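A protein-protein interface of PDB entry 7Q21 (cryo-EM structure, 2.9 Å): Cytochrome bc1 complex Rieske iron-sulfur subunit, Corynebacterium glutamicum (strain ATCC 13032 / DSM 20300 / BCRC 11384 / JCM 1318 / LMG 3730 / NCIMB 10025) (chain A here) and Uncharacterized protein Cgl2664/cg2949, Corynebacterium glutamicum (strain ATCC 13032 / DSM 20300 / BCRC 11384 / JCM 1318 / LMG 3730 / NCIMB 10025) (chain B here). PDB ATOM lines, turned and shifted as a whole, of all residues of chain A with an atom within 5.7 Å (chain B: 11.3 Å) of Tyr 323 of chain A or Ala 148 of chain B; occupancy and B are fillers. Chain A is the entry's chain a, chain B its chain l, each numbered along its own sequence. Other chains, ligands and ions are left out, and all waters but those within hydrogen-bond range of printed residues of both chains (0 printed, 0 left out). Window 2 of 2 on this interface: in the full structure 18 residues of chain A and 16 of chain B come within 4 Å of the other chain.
The backbone carbonyl oxygen (O) of Gly 150 of chain B is in hydrogen-bond range of the backbone NH (N) of Asp 325 of chain A (3.0 Å).
The backbone NH (N) of Gly 150 of chain B lies within hydrogen-bond range of the backbone carbonyl oxygen (O) of Val 170 of chain B, at 3.0 Å. The side-chain hydroxyl (OG1) of Thr 169 of chain B sits at hydrogen-bond distance from the backbone carbonyl oxygen (O) of Gly 151 of chain B, 3.3 Å away. The backbone carbonyl oxygen (O) of Pro 253 of chain A lies within hydrogen-bond range of the side-chain hydroxyl (OH) of Tyr 326 of chain A. N of Val 66 of chain B is in hydrogen-bond range of O of Thr 169 of chain B. O of Thr 69 of chain B sits at hydrogen-bond distance from OH of Tyr 149 of chain B (3.3 Å). O of Leu 68 of chain B lies within hydrogen-bond range of OH of Tyr 149 of chain B, 2.5 Å away.
O of Pro 253 of chain A touches CB of Tyr 149 of chain B, 3.4 Å away. Gly 150 of chain B touches Pro 253 of chain A. Tyr 323 of chain A touches Ala 148 of chain B. Tyr 323 of chain A touches Tyr 149 of chain B (CE1 to O, 3.5 Å). Gly 324 of chain A touches Gly 150 of chain B. OD1 of Asp 325 of chain A touches CG2 of Val 152 of chain B, at 3.3 Å. Asp 325 of chain A touches Thr 169 of chain B. Tyr 326 of chain A touches Gly 150 of chain B.
Pro 253 of chain A touches just these residues of chain B: Tyr 149 and Gly 150. No residue of chain B comes within 4 Å of His 322 of chain A. Of chain B, only Gly 150 (3.2 Å) comes within 4 Å of Gly 324 of chain A. Printed residues of chain B within 4 Å of Asp 325 of chain A: Gly 150, Val 152 and Thr 169. Tyr 326 of chain A touches just one residue of chain B: Gly 150. No residue of chain B comes within 4 Å of Ile 381 of chain A. No residue of chain B comes within 4 Å of Thr 382 of chain A. No residue of chain B comes within 4 Å of Val 383 of chain A. Asp 98 of chain B touches none of the printed residues of chain A. Of the printed residues of chain A, Thr 169 of chain B touches Asp 325 (3.8 Å). The nearest printed residue of chain A that does not touch Val 152 of chain B is Gly 324 of chain A (4.5 Å).
Along chain B the printed residues that touch a printed residue of chain A span positions 148 to 169. Among the printed residues, 9 pairs touch across the chains. Among the printed residues, no Asp or Glu carboxylate lies within 4 Å of a Lys or Arg side-chain nitrogen of the other chain.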
ATOM      1  N   PRO A 253      25.889 -19.964  17.859  1.00  0.00           N
ATOM      2  CA  PRO A 253      25.346 -20.888  16.858  1.00  0.00           C
ATOM      3  C   PRO A 253      26.348 -21.911  16.320  1.00  0.00           C
ATOM      4  O   PRO A 253      26.106 -22.518  15.278  1.00  0.00           O
ATOM      5  CB  PRO A 253      24.929 -19.924  15.741  1.00  0.00           C
ATOM      6  CG  PRO A 253      25.980 -18.842  15.810  1.00  0.00           C
ATOM      7  CD  PRO A 253      26.166 -18.630  17.294  1.00  0.00           C
ATOM      8  N   PHE A 321      10.984 -18.159  11.117  1.00  0.00           N
ATOM      9  CA  PHE A 321      11.171 -18.354  12.548  1.00  0.00           C
ATOM     10  C   PHE A 321      12.397 -19.216  12.845  1.00  0.00           C
ATOM     11  O   PHE A 321      12.703 -19.469  14.012  1.00  0.00           O
ATOM     12  CB  PHE A 321       9.926 -18.971  13.185  1.00  0.00           C
ATOM     13  CG  PHE A 321       8.822 -17.998  13.504  1.00  0.00           C
ATOM     14  CD1 PHE A 321       8.654 -16.831  12.769  1.00  0.00           C
ATOM     15  CD2 PHE A 321       7.917 -18.274  14.521  1.00  0.00           C
ATOM     16  CE1 PHE A 321       7.625 -15.947  13.061  1.00  0.00           C
ATOM     17  CE2 PHE A 321       6.886 -17.391  14.813  1.00  0.00           C
ATOM     18  CZ  PHE A 321       6.740 -16.235  14.075  1.00  0.00           C
ATOM     19  N   HIS A 322      13.091 -19.655  11.785  1.00  0.00           N
ATOM     20  CA  HIS A 322      14.252 -20.507  11.953  1.00  0.00           C
ATOM     21  C   HIS A 322      15.517 -19.747  11.562  1.00  0.00           C
ATOM     22  O   HIS A 322      15.484 -18.866  10.707  1.00  0.00           O
ATOM     23  CB  HIS A 322      14.076 -21.789  11.137  1.00  0.00           C
ATOM     24  CG  HIS A 322      14.120 -21.561   9.666  1.00  0.00           C
ATOM     25  ND1 HIS A 322      15.280 -21.726   8.933  1.00  0.00           N
ATOM     26  CD2 HIS A 322      13.171 -21.158   8.794  1.00  0.00           C
ATOM     27  CE1 HIS A 322      15.049 -21.437   7.672  1.00  0.00           C
ATOM     28  NE2 HIS A 322      13.762 -21.071   7.560  1.00  0.00           N
ATOM     29  N   TYR A 323      16.626 -20.115  12.201  1.00  0.00           N
ATOM     30  CA  TYR A 323      17.931 -19.756  11.685  1.00  0.00           C
ATOM     31  C   TYR A 323      18.306 -20.795  10.636  1.00  0.00           C
ATOM     32  O   TYR A 323      17.449 -21.572  10.218  1.00  0.00           O
ATOM     33  CB  TYR A 323      18.920 -19.574  12.833  1.00  0.00           C
ATOM     34  CG  TYR A 323      20.118 -18.724  12.488  1.00  0.00           C
ATOM     35  CD1 TYR A 323      21.411 -19.210  12.631  1.00  0.00           C
ATOM     36  CD2 TYR A 323      19.955 -17.438  11.991  1.00  0.00           C
ATOM     37  CE1 TYR A 323      22.510 -18.438  12.292  1.00  0.00           C
ATOM     38  CE2 TYR A 323      21.044 -16.645  11.663  1.00  0.00           C
ATOM     39  CZ  TYR A 323      22.327 -17.144  11.830  1.00  0.00           C
ATOM     40  OH  TYR A 323      23.413 -16.385  11.504  1.00  0.00           O
ATOM     41  N   GLY A 324      19.554 -20.736  10.158  1.00  0.00           N
ATOM     42  CA  GLY A 324      20.081 -21.668   9.172  1.00  0.00           C
ATOM     43  C   GLY A 324      19.498 -23.074   9.311  1.00  0.00           C
ATOM     44  O   GLY A 324      18.774 -23.526   8.427  1.00  0.00           O
ATOM     45  N   ASP A 325      19.795 -23.734  10.439  1.00  0.00           N
ATOM     46  CA  ASP A 325      19.373 -25.103  10.675  1.00  0.00           C
ATOM     47  C   ASP A 325      18.698 -25.250  12.038  1.00  0.00           C
ATOM     48  O   ASP A 325      18.357 -26.359  12.445  1.00  0.00           O
ATOM     49  CB  ASP A 325      20.566 -26.053  10.561  1.00  0.00           C
ATOM     50  CG  ASP A 325      20.805 -26.557   9.147  1.00  0.00           C
ATOM     51  OD1 ASP A 325      20.090 -26.116   8.228  1.00  0.00           O
ATOM     52  OD2 ASP A 325      21.684 -27.429   8.983  1.00  0.00           O
ATOM     53  N   TYR A 326      18.509 -24.128  12.739  1.00  0.00           N
ATOM     54  CA  TYR A 326      18.026 -24.155  14.110  1.00  0.00           C
ATOM     55  C   TYR A 326      16.528 -23.865  14.146  1.00  0.00           C
ATOM     56  O   TYR A 326      16.066 -22.883  13.573  1.00  0.00           O
ATOM     57  CB  TYR A 326      18.781 -23.124  14.946  1.00  0.00           C
ATOM     58  CG  TYR A 326      20.239 -23.418  15.169  1.00  0.00           C
ATOM     59  CD1 TYR A 326      20.664 -23.985  16.360  1.00  0.00           C
ATOM     60  CD2 TYR A 326      21.196 -23.101  14.214  1.00  0.00           C
ATOM     61  CE1 TYR A 326      22.005 -24.257  16.590  1.00  0.00           C
ATOM     62  CE2 TYR A 326      22.539 -23.364  14.428  1.00  0.00           C
ATOM     63  CZ  TYR A 326      22.942 -23.949  15.619  1.00  0.00           C
ATOM     64  OH  TYR A 326      24.261 -24.214  15.841  1.00  0.00           O
ATOM     65  N   TYR A 327      15.786 -24.739  14.833  1.00  0.00           N
ATOM     66  CA  TYR A 327      14.369 -24.548  15.095  1.00  0.00           C
ATOM     67  C   TYR A 327      14.142 -24.576  16.604  1.00  0.00           C
ATOM     68  O   TYR A 327      14.664 -25.452  17.289  1.00  0.00           O
ATOM     69  CB  TYR A 327      13.544 -25.627  14.388  1.00  0.00           C
ATOM     70  CG  TYR A 327      13.496 -25.507  12.885  1.00  0.00           C
ATOM     71  CD1 TYR A 327      12.374 -24.998  12.243  1.00  0.00           C
ATOM     72  CD2 TYR A 327      14.567 -25.908  12.100  1.00  0.00           C
ATOM     73  CE1 TYR A 327      12.327 -24.878  10.861  1.00  0.00           C
ATOM     74  CE2 TYR A 327      14.539 -25.792  10.719  1.00  0.00           C
ATOM     75  CZ  TYR A 327      13.410 -25.285  10.097  1.00  0.00           C
ATOM     76  OH  TYR A 327      13.393 -25.180   8.736  1.00  0.00           O
ATOM     77  N   ILE A 381      14.074 -17.060  16.137  1.00  0.00           N
ATOM     78  CA  ILE A 381      15.434 -16.895  16.626  1.00  0.00           C
ATOM     79  C   ILE A 381      16.298 -16.300  15.517  1.00  0.00           C
ATOM     80  O   ILE A 381      15.969 -16.427  14.334  1.00  0.00           O
ATOM     81  CB  ILE A 381      16.017 -18.233  17.131  1.00  0.00           C
ATOM     82  CG1 ILE A 381      15.985 -19.317  16.050  1.00  0.00           C
ATOM     83  CG2 ILE A 381      15.332 -18.687  18.406  1.00  0.00           C
ATOM     84  CD1 ILE A 381      16.898 -20.481  16.309  1.00  0.00           C
ATOM     85  N   THR A 382      17.403 -15.667  15.927  1.00  0.00           N
ATOM     86  CA  THR A 382      18.406 -15.136  15.016  1.00  0.00           C
ATOM     87  C   THR A 382      19.706 -14.918  15.782  1.00  0.00           C
ATOM     88  O   THR A 382      19.718 -15.006  17.001  1.00  0.00           O
ATOM     89  CB  THR A 382      17.945 -13.836  14.338  1.00  0.00           C
ATOM     90  OG1 THR A 382      18.865 -13.579  13.275  1.00  0.00           O
ATOM     91  CG2 THR A 382      17.850 -12.668  15.300  1.00  0.00           C
ATOM     92  N   VAL A 383      20.759 -14.524  15.056  1.00  0.00           N
ATOM     93  CA  VAL A 383      22.053 -14.269  15.668  1.00  0.00           C
ATOM     94  C   VAL A 383      22.350 -12.773  15.576  1.00  0.00           C
ATOM     95  O   VAL A 383      22.194 -12.160  14.519  1.00  0.00           O
ATOM     96  CB  VAL A 383      23.156 -15.126  15.015  1.00  0.00           C
ATOM     97  CG1 VAL A 383      24.555 -14.706  15.422  1.00  0.00           C
ATOM     98  CG2 VAL A 383      22.980 -16.601  15.306  1.00  0.00           C
ATOM     99  N   LEU A 389      23.188 -16.422  19.876  1.00  0.00           N
ATOM    100  CA  LEU A 389      21.809 -16.739  19.521  1.00  0.00           C
ATOM    101  C   LEU A 389      20.868 -15.943  20.423  1.00  0.00           C
ATOM    102  O   LEU A 389      20.996 -15.973  21.647  1.00  0.00           O
ATOM    103  CB  LEU A 389      21.578 -18.246  19.685  1.00  0.00           C
ATOM    104  CG  LEU A 389      21.838 -19.107  18.449  1.00  0.00           C
ATOM    105  CD1 LEU A 389      21.990 -20.567  18.826  1.00  0.00           C
ATOM    106  CD2 LEU A 389      20.719 -18.959  17.435  1.00  0.00           C
ATOM    107  N   THR B  65      30.900 -30.702   4.794  1.00  0.00           N
ATOM    108  CA  THR B  65      30.613 -29.435   5.447  1.00  0.00           C
ATOM    109  C   THR B  65      31.640 -28.390   5.029  1.00  0.00           C
ATOM    110  O   THR B  65      32.640 -28.700   4.378  1.00  0.00           O
ATOM    111  CB  THR B  65      30.595 -29.541   6.980  1.00  0.00           C
ATOM    112  OG1 THR B  65      31.855 -30.017   7.456  1.00  0.00           O
ATOM    113  CG2 THR B  65      29.465 -30.385   7.517  1.00  0.00           C
ATOM    114  N   VAL B  66      31.352 -27.145   5.412  1.00  0.00           N
ATOM    115  CA  VAL B  66      32.309 -26.059   5.351  1.00  0.00           C
ATOM    116  C   VAL B  66      32.783 -25.810   6.779  1.00  0.00           C
ATOM    117  O   VAL B  66      32.078 -25.181   7.569  1.00  0.00           O
ATOM    118  CB  VAL B  66      31.695 -24.807   4.691  1.00  0.00           C
ATOM    119  CG1 VAL B  66      32.664 -23.632   4.656  1.00  0.00           C
ATOM    120  CG2 VAL B  66      31.198 -25.115   3.289  1.00  0.00           C
ATOM    121  N   HIS B  67      33.961 -26.355   7.104  1.00  0.00           N
ATOM    122  CA  HIS B  67      34.576 -26.123   8.399  1.00  0.00           C
ATOM    123  C   HIS B  67      35.085 -24.690   8.478  1.00  0.00           C
ATOM    124  O   HIS B  67      35.671 -24.177   7.525  1.00  0.00           O
ATOM    125  CB  HIS B  67      35.705 -27.119   8.681  1.00  0.00           C
ATOM    126  CG  HIS B  67      35.227 -28.473   9.075  1.00  0.00           C
ATOM    127  ND1 HIS B  67      34.578 -28.720  10.269  1.00  0.00           N
ATOM    128  CD2 HIS B  67      35.314 -29.656   8.438  1.00  0.00           C
ATOM    129  CE1 HIS B  67      34.277 -30.001  10.345  1.00  0.00           C
ATOM    130  NE2 HIS B  67      34.721 -30.598   9.233  1.00  0.00           N
ATOM    131  N   LEU B  68      34.824 -24.060   9.629  1.00  0.00           N
ATOM    132  CA  LEU B  68      35.367 -22.753   9.938  1.00  0.00           C
ATOM    133  C   LEU B  68      35.812 -22.741  11.394  1.00  0.00           C
ATOM    134  O   LEU B  68      34.982 -22.715  12.299  1.00  0.00           O
ATOM    135  CB  LEU B  68      34.315 -21.674   9.658  1.00  0.00           C
ATOM    136  CG  LEU B  68      34.780 -20.239   9.895  1.00  0.00           C
ATOM    137  CD1 LEU B  68      35.865 -19.842   8.906  1.00  0.00           C
ATOM    138  CD2 LEU B  68      33.614 -19.268   9.830  1.00  0.00           C
ATOM    139  N   THR B  69      37.134 -22.757  11.594  1.00  0.00           N
ATOM    140  CA  THR B  69      37.752 -22.728  12.910  1.00  0.00           C
ATOM    141  C   THR B  69      37.314 -21.451  13.629  1.00  0.00           C
ATOM    142  O   THR B  69      37.022 -20.448  12.980  1.00  0.00           O
ATOM    143  CB  THR B  69      39.277 -22.866  12.793  1.00  0.00           C
ATOM    144  OG1 THR B  69      39.566 -24.065  12.073  1.00  0.00           O
ATOM    145  CG2 THR B  69      39.996 -22.912  14.124  1.00  0.00           C
ATOM    146  N   THR B  70      37.260 -21.518  14.966  1.00  0.00           N
ATOM    147  CA  THR B  70      36.850 -20.413  15.823  1.00  0.00           C
ATOM    148  C   THR B  70      37.585 -19.129  15.443  1.00  0.00           C
ATOM    149  O   THR B  70      36.961 -18.075  15.327  1.00  0.00           O
ATOM    150  CB  THR B  70      36.994 -20.788  17.303  1.00  0.00           C
ATOM    151  OG1 THR B  70      36.085 -21.858  17.562  1.00  0.00           O
ATOM    152  CG2 THR B  70      36.705 -19.639  18.244  1.00  0.00           C
ATOM    153  N   GLY B  72      38.809 -18.078  12.639  1.00  0.00           N
ATOM    154  CA  GLY B  72      38.675 -17.624  11.258  1.00  0.00           C
ATOM    155  C   GLY B  72      39.542 -18.375  10.247  1.00  0.00           C
ATOM    156  O   GLY B  72      40.094 -17.758   9.332  1.00  0.00           O
ATOM    157  N   ALA B  74      39.181 -21.399   7.442  1.00  0.00           N
ATOM    158  CA  ALA B  74      38.103 -22.032   6.702  1.00  0.00           C
ATOM    159  C   ALA B  74      38.629 -23.147   5.803  1.00  0.00           C
ATOM    160  O   ALA B  74      39.812 -23.183   5.459  1.00  0.00           O
ATOM    161  CB  ALA B  74      37.351 -20.997   5.905  1.00  0.00           C
ATOM    162  N   GLY B  75      37.707 -24.034   5.411  1.00  0.00           N
ATOM    163  CA  GLY B  75      37.978 -25.130   4.497  1.00  0.00           C
ATOM    164  C   GLY B  75      36.739 -25.995   4.304  1.00  0.00           C
ATOM    165  O   GLY B  75      35.692 -25.727   4.893  1.00  0.00           O
ATOM    166  N   VAL B  97      32.632 -23.298  -3.115  1.00  0.00           N
ATOM    167  CA  VAL B  97      31.700 -23.288  -2.000  1.00  0.00           C
ATOM    168  C   VAL B  97      30.505 -22.400  -2.337  1.00  0.00           C
ATOM    169  O   VAL B  97      29.388 -22.897  -2.437  1.00  0.00           O
ATOM    170  CB  VAL B  97      32.371 -22.915  -0.664  1.00  0.00           C
ATOM    171  CG1 VAL B  97      31.342 -22.713   0.431  1.00  0.00           C
ATOM    172  CG2 VAL B  97      33.361 -23.982  -0.244  1.00  0.00           C
ATOM    173  N   ASP B  98      30.741 -21.095  -2.499  1.00  0.00           N
ATOM    174  CA  ASP B  98      29.670 -20.200  -2.903  1.00  0.00           C
ATOM    175  C   ASP B  98      30.088 -19.415  -4.141  1.00  0.00           C
ATOM    176  O   ASP B  98      29.421 -19.484  -5.171  1.00  0.00           O
ATOM    177  CB  ASP B  98      29.187 -19.319  -1.748  1.00  0.00           C
ATOM    178  CG  ASP B  98      27.719 -18.940  -1.853  1.00  0.00           C
ATOM    179  OD1 ASP B  98      27.160 -19.030  -2.966  1.00  0.00           O
ATOM    180  OD2 ASP B  98      27.140 -18.566  -0.814  1.00  0.00           O
ATOM    181  N   LEU B 142      39.994 -21.783   2.323  1.00  0.00           N
ATOM    182  CA  LEU B 142      39.083 -20.782   1.786  1.00  0.00           C
ATOM    183  C   LEU B 142      39.559 -19.387   2.187  1.00  0.00           C
ATOM    184  O   LEU B 142      40.657 -19.235   2.728  1.00  0.00           O
ATOM    185  CB  LEU B 142      37.670 -21.052   2.317  1.00  0.00           C
ATOM    186  CG  LEU B 142      36.885 -22.180   1.652  1.00  0.00           C
ATOM    187  CD1 LEU B 142      35.652 -22.556   2.460  1.00  0.00           C
ATOM    188  CD2 LEU B 142      36.547 -21.835   0.212  1.00  0.00           C
ATOM    189  N   GLU B 143      38.725 -18.375   1.901  1.00  0.00           N
ATOM    190  CA  GLU B 143      39.038 -16.977   2.160  1.00  0.00           C
ATOM    191  C   GLU B 143      38.175 -16.444   3.307  1.00  0.00           C
ATOM    192  O   GLU B 143      38.393 -15.326   3.778  1.00  0.00           O
ATOM    193  CB  GLU B 143      38.881 -16.150   0.878  1.00  0.00           C
ATOM    194  CG  GLU B 143      39.694 -14.859   0.881  1.00  0.00           C
ATOM    195  CD  GLU B 143      41.212 -14.992   0.840  1.00  0.00           C
ATOM    196  OE1 GLU B 143      41.719 -15.925   0.176  1.00  0.00           O
ATOM    197  OE2 GLU B 143      41.890 -14.154   1.470  1.00  0.00           O
ATOM    198  N   ASN B 144      37.198 -17.252   3.754  1.00  0.00           N
ATOM    199  CA  ASN B 144      36.216 -16.875   4.765  1.00  0.00           C
ATOM    200  C   ASN B 144      35.547 -15.550   4.385  1.00  0.00           C
ATOM    201  O   ASN B 144      35.741 -14.542   5.067  1.00  0.00           O
ATOM    202  CB  ASN B 144      36.808 -16.885   6.184  1.00  0.00           C
ATOM    203  CG  ASN B 144      35.781 -16.729   7.291  1.00  0.00           C
ATOM    204  OD1 ASN B 144      34.588 -16.912   7.070  1.00  0.00           O
ATOM    205  ND2 ASN B 144      36.239 -16.416   8.495  1.00  0.00           N
ATOM    206  N   PRO B 145      34.751 -15.500   3.287  1.00  0.00           N
ATOM    207  CA  PRO B 145      34.077 -14.265   2.873  1.00  0.00           C
ATOM    208  C   PRO B 145      33.067 -13.763   3.904  1.00  0.00           C
ATOM    209  O   PRO B 145      32.960 -12.559   4.124  1.00  0.00           O
ATOM    210  CB  PRO B 145      33.375 -14.630   1.558  1.00  0.00           C
ATOM    211  CG  PRO B 145      33.231 -16.133   1.616  1.00  0.00           C
ATOM    212  CD  PRO B 145      34.433 -16.627   2.394  1.00  0.00           C
ATOM    213  N   GLY B 146      32.348 -14.701   4.536  1.00  0.00           N
ATOM    214  CA  GLY B 146      31.451 -14.392   5.637  1.00  0.00           C
ATOM    215  C   GLY B 146      30.394 -15.472   5.848  1.00  0.00           C
ATOM    216  O   GLY B 146      29.197 -15.191   5.775  1.00  0.00           O
ATOM    217  N   PHE B 147      30.858 -16.696   6.124  1.00  0.00           N
ATOM    218  CA  PHE B 147      29.975 -17.822   6.382  1.00  0.00           C
ATOM    219  C   PHE B 147      29.468 -17.769   7.820  1.00  0.00           C
ATOM    220  O   PHE B 147      30.234 -17.504   8.745  1.00  0.00           O
ATOM    221  CB  PHE B 147      30.680 -19.147   6.078  1.00  0.00           C
ATOM    222  CG  PHE B 147      31.058 -19.351   4.632  1.00  0.00           C
ATOM    223  CD1 PHE B 147      32.290 -19.897   4.293  1.00  0.00           C
ATOM    224  CD2 PHE B 147      30.190 -18.991   3.609  1.00  0.00           C
ATOM    225  CE1 PHE B 147      32.638 -20.090   2.962  1.00  0.00           C
ATOM    226  CE2 PHE B 147      30.538 -19.177   2.279  1.00  0.00           C
ATOM    227  CZ  PHE B 147      31.763 -19.727   1.959  1.00  0.00           C
ATOM    228  N   ALA B 148      28.166 -18.027   7.982  1.00  0.00           N
ATOM    229  CA  ALA B 148      27.533 -18.054   9.290  1.00  0.00           C
ATOM    230  C   ALA B 148      27.423 -19.493   9.779  1.00  0.00           C
ATOM    231  O   ALA B 148      26.939 -20.359   9.051  1.00  0.00           O
ATOM    232  CB  ALA B 148      26.176 -17.396   9.223  1.00  0.00           C
ATOM    233  N   TYR B 149      27.881 -19.732  11.016  1.00  0.00           N
ATOM    234  CA  TYR B 149      27.655 -20.997  11.696  1.00  0.00           C
ATOM    235  C   TYR B 149      26.161 -21.301  11.712  1.00  0.00           C
ATOM    236  O   TYR B 149      25.351 -20.434  12.034  1.00  0.00           O
ATOM    237  CB  TYR B 149      28.189 -20.959  13.129  1.00  0.00           C
ATOM    238  CG  TYR B 149      29.689 -20.950  13.258  1.00  0.00           C
ATOM    239  CD1 TYR B 149      30.335 -19.970  13.999  1.00  0.00           C
ATOM    240  CD2 TYR B 149      30.467 -21.922  12.647  1.00  0.00           C
ATOM    241  CE1 TYR B 149      31.714 -19.955  14.133  1.00  0.00           C
ATOM    242  CE2 TYR B 149      31.848 -21.920  12.768  1.00  0.00           C
ATOM    243  CZ  TYR B 149      32.472 -20.932  13.513  1.00  0.00           C
ATOM    244  OH  TYR B 149      33.829 -20.913  13.643  1.00  0.00           O
ATOM    245  N   GLY B 150      25.819 -22.533  11.319  1.00  0.00           N
ATOM    246  CA  GLY B 150      24.440 -22.990  11.297  1.00  0.00           C
ATOM    247  C   GLY B 150      23.763 -22.761   9.947  1.00  0.00           C
ATOM    248  O   GLY B 150      22.712 -23.343   9.681  1.00  0.00           O
ATOM    249  N   GLY B 151      24.371 -21.916   9.106  1.00  0.00           N
ATOM    250  CA  GLY B 151      23.874 -21.643   7.768  1.00  0.00           C
ATOM    251  C   GLY B 151      24.177 -22.788   6.807  1.00  0.00           C
ATOM    252  O   GLY B 151      24.881 -23.737   7.157  1.00  0.00           O
ATOM    253  N   VAL B 152      23.624 -22.682   5.593  1.00  0.00           N
ATOM    254  CA  VAL B 152      23.778 -23.697   4.562  1.00  0.00           C
ATOM    255  C   VAL B 152      24.244 -23.008   3.282  1.00  0.00           C
ATOM    256  O   VAL B 152      23.716 -21.961   2.911  1.00  0.00           O
ATOM    257  CB  VAL B 152      22.471 -24.488   4.342  1.00  0.00           C
ATOM    258  CG1 VAL B 152      22.655 -25.601   3.327  1.00  0.00           C
ATOM    259  CG2 VAL B 152      21.901 -25.051   5.636  1.00  0.00           C
ATOM    260  N   VAL B 153      25.231 -23.612   2.612  1.00  0.00           N
ATOM    261  CA  VAL B 153      25.841 -23.024   1.429  1.00  0.00           C
ATOM    262  C   VAL B 153      25.951 -24.088   0.337  1.00  0.00           C
ATOM    263  O   VAL B 153      26.169 -25.259   0.642  1.00  0.00           O
ATOM    264  CB  VAL B 153      27.205 -22.382   1.751  1.00  0.00           C
ATOM    265  CG1 VAL B 153      27.054 -21.088   2.537  1.00  0.00           C
ATOM    266  CG2 VAL B 153      28.139 -23.344   2.470  1.00  0.00           C
ATOM    267  N   PRO B 154      25.811 -23.724  -0.961  1.00  0.00           N
ATOM    268  CA  PRO B 154      25.798 -24.713  -2.041  1.00  0.00           C
ATOM    269  C   PRO B 154      27.168 -25.109  -2.597  1.00  0.00           C
ATOM    270  O   PRO B 154      27.603 -24.596  -3.630  1.00  0.00           O
ATOM    271  CB  PRO B 154      24.919 -24.041  -3.110  1.00  0.00           C
ATOM    272  CG  PRO B 154      24.999 -22.543  -2.838  1.00  0.00           C
ATOM    273  CD  PRO B 154      25.607 -22.355  -1.463  1.00  0.00           C
ATOM    274  N   ALA B 168      25.579 -27.718   1.979  1.00  0.00           N
ATOM    275  CA  ALA B 168      26.349 -28.176   3.125  1.00  0.00           C
ATOM    276  C   ALA B 168      26.304 -27.127   4.231  1.00  0.00           C
ATOM    277  O   ALA B 168      26.381 -25.930   3.959  1.00  0.00           O
ATOM    278  CB  ALA B 168      27.768 -28.480   2.712  1.00  0.00           C
ATOM    279  N   THR B 169      26.194 -27.606   5.475  1.00  0.00           N
ATOM    280  CA  THR B 169      26.139 -26.745   6.646  1.00  0.00           C
ATOM    281  C   THR B 169      27.521 -26.173   6.948  1.00  0.00           C
ATOM    282  O   THR B 169      28.540 -26.747   6.566  1.00  0.00           O
ATOM    283  CB  THR B 169      25.548 -27.467   7.865  1.00  0.00           C
ATOM    284  OG1 THR B 169      25.322 -26.476   8.866  1.00  0.00           O
ATOM    285  CG2 THR B 169      26.458 -28.530   8.440  1.00  0.00           C
ATOM    286  N   VAL B 170      27.529 -25.042   7.661  1.00  0.00           N
ATOM    287  CA  VAL B 170      28.760 -24.441   8.144  1.00  0.00           C
ATOM    288  C   VAL B 170      28.863 -24.725   9.639  1.00  0.00           C
ATOM    289  O   VAL B 170      27.985 -24.342  10.410  1.00  0.00           O
ATOM    290  CB  VAL B 170      28.821 -22.931   7.843  1.00  0.00           C
ATOM    291  CG1 VAL B 170      30.129 -22.317   8.316  1.00  0.00           C
ATOM    292  CG2 VAL B 170      28.600 -22.636   6.369  1.00  0.00           C
ATOM    293  N   SER B 171      29.950 -25.395  10.030  1.00  0.00           N
ATOM    294  CA  SER B 171      30.136 -25.809  11.409  1.00  0.00           C
ATOM    295  C   SER B 171      31.605 -25.711  11.803  1.00  0.00           C
ATOM    296  O   SER B 171      32.488 -25.732  10.946  1.00  0.00           O
ATOM    297  CB  SER B 171      29.588 -27.197  11.639  1.00  0.00           C
ATOM    298  OG  SER B 171      30.019 -28.084  10.618  1.00  0.00           O
ATOM    299  N   ALA B 172      31.839 -25.606  13.117  1.00  0.00           N
ATOM    300  CA  ALA B 172      33.170 -25.626  13.698  1.00  0.00           C
ATOM    301  C   ALA B 172      33.676 -27.068  13.752  1.00  0.00           C
ATOM    302  O   ALA B 172      32.880 -27.986  13.943  1.00  0.00           O
ATOM    303  CB  ALA B 172      33.131 -25.001  15.070  1.00  0.00           C
